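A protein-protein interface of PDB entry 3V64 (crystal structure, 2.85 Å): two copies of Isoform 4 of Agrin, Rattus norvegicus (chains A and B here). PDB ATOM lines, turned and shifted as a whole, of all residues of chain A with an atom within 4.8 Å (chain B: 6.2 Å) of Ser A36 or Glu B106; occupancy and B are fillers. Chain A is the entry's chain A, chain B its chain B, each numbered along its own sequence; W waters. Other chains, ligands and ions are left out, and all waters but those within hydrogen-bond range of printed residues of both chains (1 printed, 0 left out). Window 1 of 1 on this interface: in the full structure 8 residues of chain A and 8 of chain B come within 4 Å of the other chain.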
ATOM      1  N   LEU A  34      19.828 -13.969   0.952  1.00  0.00           N
ATOM      2  CA  LEU A  34      19.814 -12.530   1.197  1.00  0.00           C
ATOM      3  C   LEU A  34      20.362 -11.711   0.040  1.00  0.00           C
ATOM      4  O   LEU A  34      21.511 -11.879  -0.368  1.00  0.00           O
ATOM      5  CB  LEU A  34      20.573 -12.194   2.483  1.00  0.00           C
ATOM      6  CG  LEU A  34      20.121 -12.887   3.771  1.00  0.00           C
ATOM      7  CD1 LEU A  34      21.102 -12.568   4.887  1.00  0.00           C
ATOM      8  CD2 LEU A  34      18.706 -12.478   4.166  1.00  0.00           C
ATOM      9  N   GLN A  35      19.519 -10.825  -0.480  1.00  0.00           N
ATOM     10  CA  GLN A  35      19.901  -9.896  -1.534  1.00  0.00           C
ATOM     11  C   GLN A  35      20.679  -8.733  -0.933  1.00  0.00           C
ATOM     12  O   GLN A  35      21.581  -8.184  -1.568  1.00  0.00           O
ATOM     13  CB  GLN A  35      18.655  -9.351  -2.237  1.00  0.00           C
ATOM     14  CG  GLN A  35      17.615 -10.397  -2.612  1.00  0.00           C
ATOM     15  CD  GLN A  35      17.829 -10.990  -3.994  1.00  0.00           C
ATOM     16  OE1 GLN A  35      16.911 -11.014  -4.813  1.00  0.00           O
ATOM     17  NE2 GLN A  35      19.042 -11.468  -4.262  1.00  0.00           N
ATOM     18  N   SER A  36      20.322  -8.367   0.295  1.00  0.00           N
ATOM     19  CA  SER A  36      20.828  -7.150   0.914  1.00  0.00           C
ATOM     20  C   SER A  36      21.184  -7.313   2.384  1.00  0.00           C
ATOM     21  O   SER A  36      20.469  -7.973   3.142  1.00  0.00           O
ATOM     22  CB  SER A  36      19.808  -6.019   0.758  1.00  0.00           C
ATOM     23  OG  SER A  36      18.582  -6.344   1.394  1.00  0.00           O
ATOM     24  N   ASN A  37      22.301  -6.700   2.768  1.00  0.00           N
ATOM     25  CA  ASN A  37      22.709  -6.598   4.162  1.00  0.00           C
ATOM     26  C   ASN A  37      22.911  -5.143   4.565  1.00  0.00           C
ATOM     27  O   ASN A  37      23.455  -4.352   3.796  1.00  0.00           O
ATOM     28  CB  ASN A  37      24.008  -7.370   4.412  1.00  0.00           C
ATOM     29  CG  ASN A  37      23.846  -8.869   4.247  1.00  0.00           C
ATOM     30  OD1 ASN A  37      22.917  -9.346   3.597  1.00  0.00           O
ATOM     31  ND2 ASN A  37      24.766  -9.625   4.833  1.00  0.00           N
ATOM     32  N   HIS A  38      22.461  -4.795   5.766  1.00  0.00           N
ATOM     33  CA  HIS A  38      22.730  -3.483   6.343  1.00  0.00           C
ATOM     34  C   HIS A  38      22.799  -3.545   7.839  1.00  0.00           C
ATOM     35  O   HIS A  38      21.934  -4.136   8.489  1.00  0.00           O
ATOM     36  CB  HIS A  38      21.678  -2.468   5.918  1.00  0.00           C
ATOM     37  CG  HIS A  38      21.910  -1.084   6.478  1.00  0.00           C
ATOM     38  ND1 HIS A  38      22.719  -0.186   5.880  1.00  0.00           N
ATOM     39  CD2 HIS A  38      21.416  -0.466   7.619  1.00  0.00           C
ATOM     40  CE1 HIS A  38      22.737   0.949   6.599  1.00  0.00           C
ATOM     41  NE2 HIS A  38      21.940   0.779   7.663  1.00  0.00           N
ATOM     42  N   ARG A 105      25.174  -3.775   1.891  1.00  0.00           N
ATOM     43  CA  ARG A 105      25.389  -4.612   0.723  1.00  0.00           C
ATOM     44  C   ARG A 105      24.124  -4.703  -0.118  1.00  0.00           C
ATOM     45  O   ARG A 105      23.058  -5.052   0.385  1.00  0.00           O
ATOM     46  CB  ARG A 105      25.836  -6.017   1.133  1.00  0.00           C
ATOM     47  CG  ARG A 105      26.551  -6.782   0.031  1.00  0.00           C
ATOM     48  CD  ARG A 105      26.515  -8.285   0.263  1.00  0.00           C
ATOM     49  NE  ARG A 105      25.443  -8.934  -0.491  1.00  0.00           N
ATOM     50  CZ  ARG A 105      24.415  -9.581   0.049  1.00  0.00           C
ATOM     51  NH1 ARG A 105      24.301  -9.687   1.364  1.00  0.00           N
ATOM     52  NH2 ARG A 105      23.502 -10.133  -0.735  1.00  0.00           N
ATOM     53  N   GLU A 106      24.252  -4.364  -1.396  1.00  0.00           N
ATOM     54  CA  GLU A 106      23.222  -4.642  -2.382  1.00  0.00           C
ATOM     55  C   GLU A 106      23.792  -5.675  -3.338  1.00  0.00           C
ATOM     56  O   GLU A 106      24.658  -5.355  -4.155  1.00  0.00           O
ATOM     57  CB  GLU A 106      22.834  -3.375  -3.148  1.00  0.00           C
ATOM     58  CG  GLU A 106      22.000  -2.381  -2.356  1.00  0.00           C
ATOM     59  CD  GLU A 106      20.585  -2.863  -2.082  1.00  0.00           C
ATOM     60  OE1 GLU A 106      19.970  -2.377  -1.110  1.00  0.00           O
ATOM     61  OE2 GLU A 106      20.077  -3.721  -2.837  1.00  0.00           O
ATOM     62  N   GLN B  35      15.480  -2.456  -7.729  1.00  0.00           N
ATOM     63  CA  GLN B  35      15.538  -3.867  -7.358  1.00  0.00           C
ATOM     64  C   GLN B  35      14.619  -4.143  -6.176  1.00  0.00           C
ATOM     65  O   GLN B  35      13.815  -5.077  -6.209  1.00  0.00           O
ATOM     66  CB  GLN B  35      16.971  -4.265  -6.992  1.00  0.00           C
ATOM     67  CG  GLN B  35      17.932  -4.319  -8.166  1.00  0.00           C
ATOM     68  CD  GLN B  35      17.754  -5.569  -9.001  1.00  0.00           C
ATOM     69  OE1 GLN B  35      18.290  -6.628  -8.678  1.00  0.00           O
ATOM     70  NE2 GLN B  35      17.007  -5.450 -10.091  1.00  0.00           N
ATOM     71  N   SER B  36      14.747  -3.322  -5.137  1.00  0.00           N
ATOM     72  CA  SER B  36      13.985  -3.500  -3.909  1.00  0.00           C
ATOM     73  C   SER B  36      13.616  -2.173  -3.254  1.00  0.00           C
ATOM     74  O   SER B  36      14.332  -1.178  -3.387  1.00  0.00           O
ATOM     75  CB  SER B  36      14.761  -4.379  -2.923  1.00  0.00           C
ATOM     76  OG  SER B  36      15.947  -3.737  -2.484  1.00  0.00           O
ATOM     77  N   ASN B  37      12.489  -2.177  -2.545  1.00  0.00           N
ATOM     78  CA  ASN B  37      12.014  -1.009  -1.812  1.00  0.00           C
ATOM     79  C   ASN B  37      11.744  -1.354  -0.351  1.00  0.00           C
ATOM     80  O   ASN B  37      11.260  -2.446  -0.053  1.00  0.00           O
ATOM     81  CB  ASN B  37      10.727  -0.458  -2.438  1.00  0.00           C
ATOM     82  CG  ASN B  37      10.829  -0.267  -3.940  1.00  0.00           C
ATOM     83  OD1 ASN B  37      11.045   0.843  -4.419  1.00  0.00           O
ATOM     84  ND2 ASN B  37      10.661  -1.352  -4.691  1.00  0.00           N
ATOM     85  N   TYR B  78       1.582  -3.236  -6.043  1.00  0.00           N
ATOM     86  CA  TYR B  78       2.598  -2.815  -7.008  1.00  0.00           C
ATOM     87  C   TYR B  78       2.558  -3.584  -8.328  1.00  0.00           C
ATOM     88  O   TYR B  78       2.381  -4.802  -8.344  1.00  0.00           O
ATOM     89  CB  TYR B  78       4.007  -2.843  -6.392  1.00  0.00           C
ATOM     90  CG  TYR B  78       4.419  -4.152  -5.760  1.00  0.00           C
ATOM     91  CD1 TYR B  78       5.064  -5.136  -6.506  1.00  0.00           C
ATOM     92  CD2 TYR B  78       4.186  -4.397  -4.408  1.00  0.00           C
ATOM     93  CE1 TYR B  78       5.453  -6.332  -5.927  1.00  0.00           C
ATOM     94  CE2 TYR B  78       4.572  -5.589  -3.819  1.00  0.00           C
ATOM     95  CZ  TYR B  78       5.205  -6.552  -4.582  1.00  0.00           C
ATOM     96  OH  TYR B  78       5.583  -7.735  -3.998  1.00  0.00           O
ATOM     97  N   HIS B 104       7.897  -3.546   2.476  1.00  0.00           N
ATOM     98  CA  HIS B 104       9.132  -3.946   1.814  1.00  0.00           C
ATOM     99  C   HIS B 104       8.829  -4.823   0.637  1.00  0.00           C
ATOM    100  O   HIS B 104       7.863  -5.585   0.660  1.00  0.00           O
ATOM    101  CB  HIS B 104      10.042  -4.688   2.791  1.00  0.00           C
ATOM    102  CG  HIS B 104      11.425  -4.976   2.248  1.00  0.00           C
ATOM    103  ND1 HIS B 104      11.692  -6.050   1.479  1.00  0.00           N
ATOM    104  CD2 HIS B 104      12.625  -4.294   2.396  1.00  0.00           C
ATOM    105  CE1 HIS B 104      12.994  -6.048   1.149  1.00  0.00           C
ATOM    106  NE2 HIS B 104      13.565  -4.974   1.709  1.00  0.00           N
ATOM    107  N   ARG B 105       9.645  -4.714  -0.407  1.00  0.00           N
ATOM    108  CA  ARG B 105       9.596  -5.666  -1.510  1.00  0.00           C
ATOM    109  C   ARG B 105      10.995  -5.952  -2.051  1.00  0.00           C
ATOM    110  O   ARG B 105      11.807  -5.042  -2.211  1.00  0.00           O
ATOM    111  CB  ARG B 105       8.660  -5.186  -2.629  1.00  0.00           C
ATOM    112  CG  ARG B 105       9.377  -4.575  -3.820  1.00  0.00           C
ATOM    113  CD  ARG B 105       8.427  -4.214  -4.949  1.00  0.00           C
ATOM    114  NE  ARG B 105       9.137  -3.463  -5.978  1.00  0.00           N
ATOM    115  CZ  ARG B 105       9.748  -4.016  -7.022  1.00  0.00           C
ATOM    116  NH1 ARG B 105       9.728  -5.328  -7.195  1.00  0.00           N
ATOM    117  NH2 ARG B 105      10.381  -3.253  -7.899  1.00  0.00           N
ATOM    118  N   GLU B 106      11.267  -7.228  -2.301  1.00  0.00           N
ATOM    119  CA  GLU B 106      12.477  -7.658  -2.990  1.00  0.00           C
ATOM    120  C   GLU B 106      12.051  -8.365  -4.262  1.00  0.00           C
ATOM    121  O   GLU B 106      11.481  -9.460  -4.208  1.00  0.00           O
ATOM    122  CB  GLU B 106      13.301  -8.599  -2.112  1.00  0.00           C
ATOM    123  CG  GLU B 106      14.265  -7.890  -1.176  1.00  0.00           C
ATOM    124  CD  GLU B 106      14.874  -8.812  -0.136  1.00  0.00           C
ATOM    125  OE1 GLU B 106      14.506 -10.008  -0.090  1.00  0.00           O
ATOM    126  OE2 GLU B 106      15.721  -8.335   0.648  1.00  0.00           O
ATOM    127  N   HIS B 107      12.328  -7.734  -5.402  1.00  0.00           N
ATOM    128  CA  HIS B 107      11.792  -8.170  -6.692  1.00  0.00           C
ATOM    129  C   HIS B 107      10.301  -8.368  -6.591  1.00  0.00           C
ATOM    130  O   HIS B 107       9.579  -7.467  -6.160  1.00  0.00           O
ATOM    131  CB  HIS B 107      12.483  -9.440  -7.191  1.00  0.00           C
ATOM    132  CG  HIS B 107      13.967  -9.286  -7.411  1.00  0.00           C
ATOM    133  ND1 HIS B 107      14.488  -8.336  -8.214  1.00  0.00           N
ATOM    134  CD2 HIS B 107      15.040 -10.012  -6.914  1.00  0.00           C
ATOM    135  CE1 HIS B 107      15.827  -8.444  -8.221  1.00  0.00           C
ATOM    136  NE2 HIS B 107      16.166  -9.469  -7.426  1.00  0.00           N
ATOM    137  N   ARG B 108       9.833  -9.554  -6.965  1.00  0.00           N
ATOM    138  CA  ARG B 108       8.409  -9.879  -6.924  1.00  0.00           C
ATOM    139  C   ARG B 108       7.868  -9.957  -5.500  1.00  0.00           C
ATOM    140  O   ARG B 108       6.774  -9.465  -5.221  1.00  0.00           O
ATOM    141  CB  ARG B 108       8.147 -11.200  -7.639  1.00  0.00           C
ATOM    142  CG  ARG B 108       8.385 -11.172  -9.139  1.00  0.00           C
ATOM    143  CD  ARG B 108       8.313 -12.581  -9.693  1.00  0.00           C
ATOM    144  NE  ARG B 108       7.087 -13.255  -9.269  1.00  0.00           N
ATOM    145  CZ  ARG B 108       6.985 -14.555  -9.010  1.00  0.00           C
ATOM    146  NH1 ARG B 108       8.041 -15.351  -9.123  1.00  0.00           N
ATOM    147  NH2 ARG B 108       5.820 -15.062  -8.627  1.00  0.00           N
ATOM    148  N   GLU B 109       8.638 -10.582  -4.612  1.00  0.00           N
ATOM    149  CA  GLU B 109       8.233 -10.789  -3.223  1.00  0.00           C
ATOM    150  C   GLU B 109       8.164  -9.474  -2.459  1.00  0.00           C
ATOM    151  O   GLU B 109       9.100  -8.676  -2.495  1.00  0.00           O
ATOM    152  CB  GLU B 109       9.204 -11.738  -2.517  1.00  0.00           C
ATOM    153  CG  GLU B 109       9.311 -13.116  -3.150  1.00  0.00           C
ATOM    154  CD  GLU B 109      10.716 -13.682  -3.085  1.00  0.00           C
ATOM    155  OE1 GLU B 109      11.678 -12.942  -3.392  1.00  0.00           O
ATOM    156  OE2 GLU B 109      10.862 -14.872  -2.736  1.00  0.00           O
ATOM    157  N   GLY B 110       7.045  -9.261  -1.775  1.00  0.00           N
ATOM    158  CA  GLY B 110       6.843  -8.071  -0.960  1.00  0.00           C
ATOM    159  C   GLY B 110       6.071  -8.392   0.302  1.00  0.00           C
ATOM    160  O   GLY B 110       5.358  -9.397   0.363  1.00  0.00           O
ATOM    161  N   THR B 129      10.629  -8.139 -12.651  1.00  0.00           N
ATOM    162  CA  THR B 129      11.002  -8.148 -11.235  1.00  0.00           C
ATOM    163  C   THR B 129      11.479  -6.774 -10.761  1.00  0.00           C
ATOM    164  O   THR B 129      11.912  -6.618  -9.616  1.00  0.00           O
ATOM    165  CB  THR B 129      12.119  -9.178 -10.955  1.00  0.00           C
ATOM    166  OG1 THR B 129      13.182  -9.003 -11.901  1.00  0.00           O
ATOM    167  CG2 THR B 129      11.582 -10.602 -11.059  1.00  0.00           C
ATOM    168  N   HIS B 170      17.209   2.584   4.075  1.00  0.00           N
ATOM    169  CA  HIS B 170      17.857   2.684   5.384  1.00  0.00           C
ATOM    170  C   HIS B 170      18.090   4.115   5.800  1.00  0.00           C
ATOM    171  O   HIS B 170      18.636   4.374   6.876  1.00  0.00           O
ATOM    172  CB  HIS B 170      19.162   1.893   5.406  1.00  0.00           C
ATOM    173  CG  HIS B 170      18.991   0.435   5.065  1.00  0.00           C
ATOM    174  ND1 HIS B 170      18.531  -0.469   5.954  1.00  0.00           N
ATOM    175  CD2 HIS B 170      19.223  -0.257   3.886  1.00  0.00           C
ATOM    176  CE1 HIS B 170      18.478  -1.679   5.371  1.00  0.00           C
ATOM    177  NE2 HIS B 170      18.903  -1.551   4.107  1.00  0.00           N
HETATM  178  O   HOH W   1      17.197 -10.732   0.848  1.00  0.00           O
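Ser A36 touches Glu B106.
His A38 touches His B170 (CD2 to ND1, 3.3 Å).
ND1 of His B107 lies close to O of Thr B129, at 3.4 Å.
O of Gln A35 is in hydrogen-bond range of NH2 of Arg A105, 2.9 Å away.
The backbone carbonyl oxygen (O) of Gln B35 is in hydrogen-bond range of the backbone NH (N) of His B107, at 3.1 Å.
Water W1 lies within hydrogen-bond range of N of Gln A35 (2.7 Å) and OE2 of Glu B106 (2.8 Å).
Of the printed residues of chain B, Ser A36 touches Glu B106.
Printed residues of chain B within 4 Å of His A38: His B170.
Of the printed residues of chain A, Glu B106 touches Ser A36 (3.6 Å).
Of the printed residues of chain A, His B107 touches Gln A35.
Printed residues of chain A within 4 Å of His B170: His A38 (3.3 Å).
The nearest residue of chain B that does not touch Ser A36 is His B104 (5.2 Å).
Ser A36 touches Glu B106, but with the chains exchanged Glu A106 does not touch Ser B36 (4.1 Å).
Positions printed for both chains: 35, 36, 37, 105 and 106.
Of the 3 pairs that touch across the chains among the printed residues, none has its exchanged pair printed and touching as well.
The side-chain amide oxygen (OE1) of Gln A35 lies close to a ring nitrogen (NE2) of His B107, at 3.1 Å.
Printed residues of chain B that touch a printed residue of chain A: Glu B106, His B107 and His B170.
Hydrophobic or aromatic side chains of chain B that line the printed part of chain A: His B107 and His B170.
Among the printed residues, no Asp or Glu carboxylate lies within 4 Å of a Lys or Arg side-chain nitrogen of the other chain.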
